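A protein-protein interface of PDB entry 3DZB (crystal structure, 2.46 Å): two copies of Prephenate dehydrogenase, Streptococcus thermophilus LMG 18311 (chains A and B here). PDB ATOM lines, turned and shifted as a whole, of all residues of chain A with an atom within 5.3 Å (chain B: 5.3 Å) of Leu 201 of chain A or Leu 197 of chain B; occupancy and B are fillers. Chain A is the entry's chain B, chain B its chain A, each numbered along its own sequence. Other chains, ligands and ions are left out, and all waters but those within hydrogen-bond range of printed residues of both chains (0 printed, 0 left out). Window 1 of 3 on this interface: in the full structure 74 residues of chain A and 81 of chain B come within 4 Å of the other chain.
Among the printed residues, merely in contact across the chains: Gln 204 of chain A with Phe 193 of chain B, Gln 204 of chain A with Phe 255 of chain B, Phe 255 of chain A with Leu 197 of chain B, Phe 255 of chain A with Leu 201 of chain B, Leu 197 of chain A with Phe 255 of chain B, Ala 205 of chain A with Gln 189 of chain B, Leu 201 of chain A with Phe 255 of chain B, Met 226 of chain A with Ala 198 of chain B, Phe 255 of chain A with Gly 200 of chain B, Gly 200 of chain A with Phe 255 of chain B, Leu 201 of chain A with Leu 197 of chain B and Leu 197 of chain A with Leu 201 of chain B.
Leu 201 of chain A touches two residues of chain B.
Of the printed residues of chain B, Gln 204 of chain A touches Gln 189 (3.1 Å), Phe 193 (3.3 Å) and Phe 255 (3.5 Å).
Printed residues of chain A within 4 Å of Phe 193 of chain B: Gln 204 (3.3 Å).
Of the printed residues of chain A, Pro 194 of chain B touches Met 226 (3.7 Å).
His 195 of chain B touches none of the printed residues of chain A.
Of chain A, only Leu 201 and Phe 255 come within 4 Å of Leu 197 of chain B.
Of the printed residues of chain A, Gly 200 of chain B touches Phe 255 (3.7 Å).
Of the printed residues of chain A, Phe 255 of chain B touches Leu 197, Gly 200, Leu 201 and Gln 204.
The nearest residue of chain B that does not touch Leu 201 of chain A is Gln 189 of chain B (4.2 Å).
The nearest residue of chain A that does not touch Leu 197 of chain B is Met 226 of chain A (4.1 Å).
Leu 197 of chain A touches Leu 201 of chain B, and with the chains exchanged Leu 201 of chain A touches Leu 197 of chain B.
Leu 197 of chain A touches Phe 255 of chain B, and with the chains exchanged Phe 255 of chain A touches Leu 197 of chain B.
Gly 200 of chain A touches Phe 255 of chain B, and with the chains exchanged Phe 255 of chain A touches Gly 200 of chain B.
Leu 201 of chain A touches Phe 255 of chain B, and with the chains exchanged Phe 255 of chain A touches Leu 201 of chain B.
Positions printed for both chains: 196, 197, 198, 199, 200, 201, 202 and 255.
Of the 14 pairs that touch across the chains among the printed residues, 8 have their exchanged pair printed and touching as well.
The side-chain amide nitrogen of Gln 189 of chain B lies within hydrogen-bond range of the side-chain amide oxygen of Gln 204 of chain A.
SD of Met 226 of chain A sits close to O of Pro 194 of chain B, 3.7 Å away.
Of the 16 printed residues of chain A, 7 touch a printed residue of chain B.
Hydrophobic or aromatic side chains of chain A within 4 Å of the printed part of chain B: Leu 197, Leu 201, Met 226 and Phe 255.
Of the 12 printed residues of chain B, 8 touch a printed residue of chain A.
Printed residues of chain B that touch a printed residue of chain A: Gln 189, Phe 193, Pro 194, Leu 197, Ala 198, Gly 200, Leu 201 and Phe 255.
Hydrophobic or aromatic side chains of chain B within 4 Å of the printed part of chain A: Phe 193, Leu 197, Ala 198, Leu 201 and Phe 255.
Along chain B the printed residues that touch a printed residue of chain A span positions 189 to 255.
Among the printed residues, 14 pairs touch across the chains.
Among the printed residues, no Asp or Glu carboxylate lies within 4 Å of a Lys or Arg side-chain nitrogen of the other chain.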
ATOM      1  N   LEU A 196     -20.495   0.094   9.349  1.00  0.00           N
ATOM      2  CA  LEU A 196     -19.718  -0.754   8.471  1.00  0.00           C
ATOM      3  C   LEU A 196     -20.597  -1.840   7.853  1.00  0.00           C
ATOM      4  O   LEU A 196     -20.466  -2.122   6.666  1.00  0.00           O
ATOM      5  CB  LEU A 196     -18.559  -1.387   9.243  1.00  0.00           C
ATOM      6  CG  LEU A 196     -17.711  -2.441   8.514  1.00  0.00           C
ATOM      7  CD1 LEU A 196     -17.631  -2.140   7.034  1.00  0.00           C
ATOM      8  CD2 LEU A 196     -16.330  -2.479   9.115  1.00  0.00           C
ATOM      9  N   LEU A 197     -21.496  -2.429   8.642  1.00  0.00           N
ATOM     10  CA  LEU A 197     -22.378  -3.475   8.136  1.00  0.00           C
ATOM     11  C   LEU A 197     -23.395  -2.902   7.175  1.00  0.00           C
ATOM     12  O   LEU A 197     -23.739  -3.525   6.176  1.00  0.00           O
ATOM     13  CB  LEU A 197     -23.122  -4.185   9.278  1.00  0.00           C
ATOM     14  CG  LEU A 197     -22.286  -4.997  10.274  1.00  0.00           C
ATOM     15  CD1 LEU A 197     -23.207  -5.536  11.379  1.00  0.00           C
ATOM     16  CD2 LEU A 197     -21.536  -6.134   9.548  1.00  0.00           C
ATOM     17  N   ALA A 198     -23.881  -1.709   7.481  1.00  0.00           N
ATOM     18  CA  ALA A 198     -24.866  -1.065   6.631  1.00  0.00           C
ATOM     19  C   ALA A 198     -24.295  -0.797   5.258  1.00  0.00           C
ATOM     20  O   ALA A 198     -24.900  -1.147   4.248  1.00  0.00           O
ATOM     21  CB  ALA A 198     -25.333   0.242   7.257  1.00  0.00           C
ATOM     22  N   SER A 199     -23.127  -0.169   5.220  1.00  0.00           N
ATOM     23  CA  SER A 199     -22.502   0.165   3.952  1.00  0.00           C
ATOM     24  C   SER A 199     -22.183  -1.124   3.221  1.00  0.00           C
ATOM     25  O   SER A 199     -22.417  -1.242   2.022  1.00  0.00           O
ATOM     26  CB  SER A 199     -21.230   0.968   4.207  1.00  0.00           C
ATOM     27  OG  SER A 199     -21.488   2.008   5.138  1.00  0.00           O
ATOM     28  N   GLY A 200     -21.666  -2.099   3.961  1.00  0.00           N
ATOM     29  CA  GLY A 200     -21.335  -3.380   3.367  1.00  0.00           C
ATOM     30  C   GLY A 200     -22.528  -4.080   2.738  1.00  0.00           C
ATOM     31  O   GLY A 200     -22.414  -4.633   1.649  1.00  0.00           O
ATOM     32  N   LEU A 201     -23.672  -4.071   3.416  1.00  0.00           N
ATOM     33  CA  LEU A 201     -24.866  -4.720   2.895  1.00  0.00           C
ATOM     34  C   LEU A 201     -25.293  -4.040   1.599  1.00  0.00           C
ATOM     35  O   LEU A 201     -25.605  -4.703   0.608  1.00  0.00           O
ATOM     36  CB  LEU A 201     -26.000  -4.655   3.926  1.00  0.00           C
ATOM     37  CG  LEU A 201     -27.347  -5.226   3.479  1.00  0.00           C
ATOM     38  CD1 LEU A 201     -27.173  -6.678   3.083  1.00  0.00           C
ATOM     39  CD2 LEU A 201     -28.378  -5.091   4.598  1.00  0.00           C
ATOM     40  N   MET A 202     -25.289  -2.713   1.609  1.00  0.00           N
ATOM     41  CA  MET A 202     -25.660  -1.931   0.438  1.00  0.00           C
ATOM     42  C   MET A 202     -24.720  -2.269  -0.719  1.00  0.00           C
ATOM     43  O   MET A 202     -25.154  -2.585  -1.824  1.00  0.00           O
ATOM     44  CB  MET A 202     -25.563  -0.441   0.767  1.00  0.00           C
ATOM     45  CG  MET A 202     -26.173   0.468  -0.269  1.00  0.00           C
ATOM     46  SD  MET A 202     -28.095   0.313  -0.326  1.00  0.00           S
ATOM     47  CE  MET A 202     -28.278  -0.341  -2.137  1.00  0.00           C
ATOM     48  N   GLU A 203     -23.425  -2.191  -0.447  1.00  0.00           N
ATOM     49  CA  GLU A 203     -22.403  -2.500  -1.430  1.00  0.00           C
ATOM     50  C   GLU A 203     -22.743  -3.862  -2.012  1.00  0.00           C
ATOM     51  O   GLU A 203     -22.746  -4.049  -3.225  1.00  0.00           O
ATOM     52  CB  GLU A 203     -21.041  -2.531  -0.739  1.00  0.00           C
ATOM     53  CG  GLU A 203     -19.871  -2.974  -1.599  1.00  0.00           C
ATOM     54  CD  GLU A 203     -18.576  -3.114  -0.793  1.00  0.00           C
ATOM     55  OE1 GLU A 203     -18.427  -4.099  -0.033  1.00  0.00           O
ATOM     56  OE2 GLU A 203     -17.709  -2.223  -0.916  1.00  0.00           O
ATOM     57  N   GLN A 204     -23.074  -4.808  -1.142  1.00  0.00           N
ATOM     58  CA  GLN A 204     -23.407  -6.153  -1.593  1.00  0.00           C
ATOM     59  C   GLN A 204     -24.634  -6.209  -2.487  1.00  0.00           C
ATOM     60  O   GLN A 204     -24.572  -6.718  -3.606  1.00  0.00           O
ATOM     61  CB  GLN A 204     -23.620  -7.095  -0.400  1.00  0.00           C
ATOM     62  CG  GLN A 204     -23.815  -8.548  -0.820  1.00  0.00           C
ATOM     63  CD  GLN A 204     -24.042  -9.480   0.345  1.00  0.00           C
ATOM     64  OE1 GLN A 204     -25.047  -9.391   1.039  1.00  0.00           O
ATOM     65  NE2 GLN A 204     -23.105 -10.381   0.568  1.00  0.00           N
ATOM     66  N   ALA A 205     -25.748  -5.688  -1.992  1.00  0.00           N
ATOM     67  CA  ALA A 205     -27.001  -5.709  -2.739  1.00  0.00           C
ATOM     68  C   ALA A 205     -26.952  -4.980  -4.088  1.00  0.00           C
ATOM     69  O   ALA A 205     -27.610  -5.393  -5.028  1.00  0.00           O
ATOM     70  CB  ALA A 205     -28.129  -5.148  -1.875  1.00  0.00           C
ATOM     71  N   ALA A 206     -26.183  -3.897  -4.181  1.00  0.00           N
ATOM     72  CA  ALA A 206     -26.067  -3.157  -5.442  1.00  0.00           C
ATOM     73  C   ALA A 206     -25.333  -3.997  -6.494  1.00  0.00           C
ATOM     74  O   ALA A 206     -25.781  -4.090  -7.639  1.00  0.00           O
ATOM     75  CB  ALA A 206     -25.346  -1.841  -5.215  1.00  0.00           C
ATOM     76  N   PHE A 223     -34.708  -4.127   4.450  1.00  0.00           N
ATOM     77  CA  PHE A 223     -33.494  -3.703   3.781  1.00  0.00           C
ATOM     78  C   PHE A 223     -33.299  -2.204   3.974  1.00  0.00           C
ATOM     79  O   PHE A 223     -32.190  -1.741   4.237  1.00  0.00           O
ATOM     80  CB  PHE A 223     -33.574  -4.012   2.298  1.00  0.00           C
ATOM     81  CG  PHE A 223     -32.292  -3.780   1.582  1.00  0.00           C
ATOM     82  CD1 PHE A 223     -31.220  -4.646   1.762  1.00  0.00           C
ATOM     83  CD2 PHE A 223     -32.137  -2.673   0.750  1.00  0.00           C
ATOM     84  CE1 PHE A 223     -30.015  -4.415   1.125  1.00  0.00           C
ATOM     85  CE2 PHE A 223     -30.940  -2.431   0.112  1.00  0.00           C
ATOM     86  CZ  PHE A 223     -29.873  -3.302   0.294  1.00  0.00           C
ATOM     87  N   MET A 226     -32.093  -1.596   7.297  1.00  0.00           N
ATOM     88  CA  MET A 226     -30.779  -2.220   7.428  1.00  0.00           C
ATOM     89  C   MET A 226     -29.709  -1.397   6.719  1.00  0.00           C
ATOM     90  O   MET A 226     -28.522  -1.662   6.864  1.00  0.00           O
ATOM     91  CB  MET A 226     -30.766  -3.612   6.792  1.00  0.00           C
ATOM     92  CG  MET A 226     -31.522  -4.694   7.520  1.00  0.00           C
ATOM     93  SD  MET A 226     -30.739  -5.141   9.214  1.00  0.00           S
ATOM     94  CE  MET A 226     -28.877  -5.295   8.718  1.00  0.00           C
ATOM     95  N   THR A 227     -30.112  -0.400   5.945  1.00  0.00           N
ATOM     96  CA  THR A 227     -29.110   0.351   5.217  1.00  0.00           C
ATOM     97  C   THR A 227     -29.125   1.865   5.299  1.00  0.00           C
ATOM     98  O   THR A 227     -28.201   2.494   4.784  1.00  0.00           O
ATOM     99  CB  THR A 227     -29.152  -0.018   3.722  1.00  0.00           C
ATOM    100  OG1 THR A 227     -30.482   0.183   3.231  1.00  0.00           O
ATOM    101  CG2 THR A 227     -28.736  -1.466   3.509  1.00  0.00           C
ATOM    102  N   PHE A 255     -17.770 -11.149  14.269  1.00  0.00           N
ATOM    103  CA  PHE A 255     -18.970 -11.284  13.461  1.00  0.00           C
ATOM    104  C   PHE A 255     -18.860 -12.433  12.459  1.00  0.00           C
ATOM    105  O   PHE A 255     -19.835 -13.146  12.221  1.00  0.00           O
ATOM    106  CB  PHE A 255     -19.275  -9.983  12.721  1.00  0.00           C
ATOM    107  CG  PHE A 255     -20.707  -9.875  12.276  1.00  0.00           C
ATOM    108  CD1 PHE A 255     -21.712  -9.614  13.198  1.00  0.00           C
ATOM    109  CD2 PHE A 255     -21.059 -10.078  10.947  1.00  0.00           C
ATOM    110  CE1 PHE A 255     -23.055  -9.556  12.802  1.00  0.00           C
ATOM    111  CE2 PHE A 255     -22.390 -10.024  10.550  1.00  0.00           C
ATOM    112  CZ  PHE A 255     -23.393  -9.761  11.484  1.00  0.00           C
ATOM    113  N   LEU A 259     -21.196 -15.703  11.812  1.00  0.00           N
ATOM    114  CA  LEU A 259     -21.723 -16.049  10.489  1.00  0.00           C
ATOM    115  C   LEU A 259     -21.411 -17.502  10.157  1.00  0.00           C
ATOM    116  O   LEU A 259     -22.283 -18.238   9.700  1.00  0.00           O
ATOM    117  CB  LEU A 259     -21.137 -15.147   9.396  1.00  0.00           C
ATOM    118  CG  LEU A 259     -21.583 -13.688   9.384  1.00  0.00           C
ATOM    119  CD1 LEU A 259     -21.050 -13.021   8.149  1.00  0.00           C
ATOM    120  CD2 LEU A 259     -23.094 -13.597   9.407  1.00  0.00           C
ATOM    121  N   GLN B 189     -31.171 -11.915  -0.800  1.00  0.00           N
ATOM    122  CA  GLN B 189     -30.318 -10.733  -0.799  1.00  0.00           C
ATOM    123  C   GLN B 189     -30.956  -9.527  -0.125  1.00  0.00           C
ATOM    124  O   GLN B 189     -30.267  -8.783   0.560  1.00  0.00           O
ATOM    125  CB  GLN B 189     -29.910 -10.362  -2.234  1.00  0.00           C
ATOM    126  CG  GLN B 189     -29.118  -9.068  -2.342  1.00  0.00           C
ATOM    127  CD  GLN B 189     -27.763  -9.149  -1.665  1.00  0.00           C
ATOM    128  OE1 GLN B 189     -26.743  -9.409  -2.310  1.00  0.00           O
ATOM    129  NE2 GLN B 189     -27.745  -8.938  -0.361  1.00  0.00           N
ATOM    130  N   PHE B 193     -31.090 -12.761   4.175  1.00  0.00           N
ATOM    131  CA  PHE B 193     -29.749 -12.534   4.724  1.00  0.00           C
ATOM    132  C   PHE B 193     -29.781 -11.285   5.625  1.00  0.00           C
ATOM    133  O   PHE B 193     -29.156 -11.246   6.692  1.00  0.00           O
ATOM    134  CB  PHE B 193     -28.724 -12.368   3.601  1.00  0.00           C
ATOM    135  CG  PHE B 193     -27.323 -12.111   4.089  1.00  0.00           C
ATOM    136  CD1 PHE B 193     -26.734 -12.952   5.024  1.00  0.00           C
ATOM    137  CD2 PHE B 193     -26.582 -11.047   3.594  1.00  0.00           C
ATOM    138  CE1 PHE B 193     -25.424 -12.740   5.457  1.00  0.00           C
ATOM    139  CE2 PHE B 193     -25.268 -10.832   4.022  1.00  0.00           C
ATOM    140  CZ  PHE B 193     -24.691 -11.680   4.955  1.00  0.00           C
ATOM    141  N   PRO B 194     -30.489 -10.233   5.190  1.00  0.00           N
ATOM    142  CA  PRO B 194     -30.563  -9.030   6.019  1.00  0.00           C
ATOM    143  C   PRO B 194     -31.154  -9.370   7.398  1.00  0.00           C
ATOM    144  O   PRO B 194     -30.827  -8.732   8.398  1.00  0.00           O
ATOM    145  CB  PRO B 194     -31.469  -8.121   5.202  1.00  0.00           C
ATOM    146  CG  PRO B 194     -31.052  -8.451   3.804  1.00  0.00           C
ATOM    147  CD  PRO B 194     -30.958  -9.958   3.820  1.00  0.00           C
ATOM    148  N   HIS B 195     -32.033 -10.365   7.453  1.00  0.00           N
ATOM    149  CA  HIS B 195     -32.617 -10.762   8.733  1.00  0.00           C
ATOM    150  C   HIS B 195     -31.567 -11.488   9.567  1.00  0.00           C
ATOM    151  O   HIS B 195     -31.494 -11.305  10.775  1.00  0.00           O
ATOM    152  CB  HIS B 195     -33.831 -11.662   8.523  1.00  0.00           C
ATOM    153  CG  HIS B 195     -35.124 -10.911   8.439  1.00  0.00           C
ATOM    154  ND1 HIS B 195     -36.051 -10.911   9.457  1.00  0.00           N
ATOM    155  CD2 HIS B 195     -35.641 -10.128   7.459  1.00  0.00           C
ATOM    156  CE1 HIS B 195     -37.086 -10.168   9.106  1.00  0.00           C
ATOM    157  NE2 HIS B 195     -36.864  -9.683   7.898  1.00  0.00           N
ATOM    158  N   LEU B 196     -30.762 -12.312   8.907  1.00  0.00           N
ATOM    159  CA  LEU B 196     -29.688 -13.031   9.565  1.00  0.00           C
ATOM    160  C   LEU B 196     -28.676 -12.022  10.138  1.00  0.00           C
ATOM    161  O   LEU B 196     -28.216 -12.180  11.272  1.00  0.00           O
ATOM    162  CB  LEU B 196     -29.017 -13.979   8.565  1.00  0.00           C
ATOM    163  CG  LEU B 196     -27.600 -14.482   8.788  1.00  0.00           C
ATOM    164  CD1 LEU B 196     -27.449 -15.095  10.160  1.00  0.00           C
ATOM    165  CD2 LEU B 196     -27.296 -15.504   7.743  1.00  0.00           C
ATOM    166  N   LEU B 197     -28.342 -10.986   9.369  1.00  0.00           N
ATOM    167  CA  LEU B 197     -27.399  -9.975   9.844  1.00  0.00           C
ATOM    168  C   LEU B 197     -27.954  -9.232  11.057  1.00  0.00           C
ATOM    169  O   LEU B 197     -27.229  -8.981  12.008  1.00  0.00           O
ATOM    170  CB  LEU B 197     -27.076  -8.951   8.747  1.00  0.00           C
ATOM    171  CG  LEU B 197     -26.225  -9.400   7.557  1.00  0.00           C
ATOM    172  CD1 LEU B 197     -26.242  -8.319   6.488  1.00  0.00           C
ATOM    173  CD2 LEU B 197     -24.818  -9.683   8.005  1.00  0.00           C
ATOM    174  N   ALA B 198     -29.237  -8.875  11.027  1.00  0.00           N
ATOM    175  CA  ALA B 198     -29.831  -8.164  12.154  1.00  0.00           C
ATOM    176  C   ALA B 198     -29.806  -9.007  13.429  1.00  0.00           C
ATOM    177  O   ALA B 198     -29.528  -8.484  14.517  1.00  0.00           O
ATOM    178  CB  ALA B 198     -31.256  -7.738  11.831  1.00  0.00           C
ATOM    179  N   SER B 199     -30.082 -10.305  13.306  1.00  0.00           N
ATOM    180  CA  SER B 199     -30.073 -11.187  14.479  1.00  0.00           C
ATOM    181  C   SER B 199     -28.651 -11.458  14.962  1.00  0.00           C
ATOM    182  O   SER B 199     -28.403 -11.564  16.168  1.00  0.00           O
ATOM    183  CB  SER B 199     -30.780 -12.495  14.164  1.00  0.00           C
ATOM    184  OG  SER B 199     -32.107 -12.228  13.742  1.00  0.00           O
ATOM    185  N   GLY B 200     -27.716 -11.555  14.023  1.00  0.00           N
ATOM    186  CA  GLY B 200     -26.336 -11.787  14.395  1.00  0.00           C
ATOM    187  C   GLY B 200     -25.764 -10.605  15.163  1.00  0.00           C
ATOM    188  O   GLY B 200     -25.057 -10.782  16.143  1.00  0.00           O
ATOM    189  N   LEU B 201     -26.092  -9.399  14.716  1.00  0.00           N
ATOM    190  CA  LEU B 201     -25.617  -8.165  15.332  1.00  0.00           C
ATOM    191  C   LEU B 201     -26.220  -7.953  16.710  1.00  0.00           C
ATOM    192  O   LEU B 201     -25.547  -7.465  17.612  1.00  0.00           O
ATOM    193  CB  LEU B 201     -25.946  -6.966  14.430  1.00  0.00           C
ATOM    194  CG  LEU B 201     -25.788  -5.562  15.031  1.00  0.00           C
ATOM    195  CD1 LEU B 201     -24.368  -5.365  15.619  1.00  0.00           C
ATOM    196  CD2 LEU B 201     -26.083  -4.531  13.943  1.00  0.00           C
ATOM    197  N   MET B 202     -27.490  -8.306  16.873  1.00  0.00           N
ATOM    198  CA  MET B 202     -28.141  -8.152  18.167  1.00  0.00           C
ATOM    199  C   MET B 202     -27.441  -9.084  19.138  1.00  0.00           C
ATOM    200  O   MET B 202     -27.065  -8.704  20.249  1.00  0.00           O
ATOM    201  CB  MET B 202     -29.619  -8.528  18.076  1.00  0.00           C
ATOM    202  CG  MET B 202     -30.391  -8.263  19.352  1.00  0.00           C
ATOM    203  SD  MET B 202     -30.215  -6.429  19.976  1.00  0.00           S
ATOM    204  CE  MET B 202     -31.595  -5.635  18.952  1.00  0.00           C
ATOM    205  N   PHE B 255     -20.211 -11.834   1.916  1.00  0.00           N
ATOM    206  CA  PHE B 255     -20.120 -10.832   2.970  1.00  0.00           C
ATOM    207  C   PHE B 255     -18.801 -10.918   3.719  1.00  0.00           C
ATOM    208  O   PHE B 255     -18.183  -9.902   3.998  1.00  0.00           O
ATOM    209  CB  PHE B 255     -21.282 -10.962   3.970  1.00  0.00           C
ATOM    210  CG  PHE B 255     -21.631  -9.665   4.644  1.00  0.00           C
ATOM    211  CD1 PHE B 255     -22.250  -8.644   3.929  1.00  0.00           C
ATOM    212  CD2 PHE B 255     -21.299  -9.447   5.978  1.00  0.00           C
ATOM    213  CE1 PHE B 255     -22.534  -7.421   4.529  1.00  0.00           C
ATOM    214  CE2 PHE B 255     -21.574  -8.228   6.598  1.00  0.00           C
ATOM    215  CZ  PHE B 255     -22.197  -7.204   5.874  1.00  0.00           C
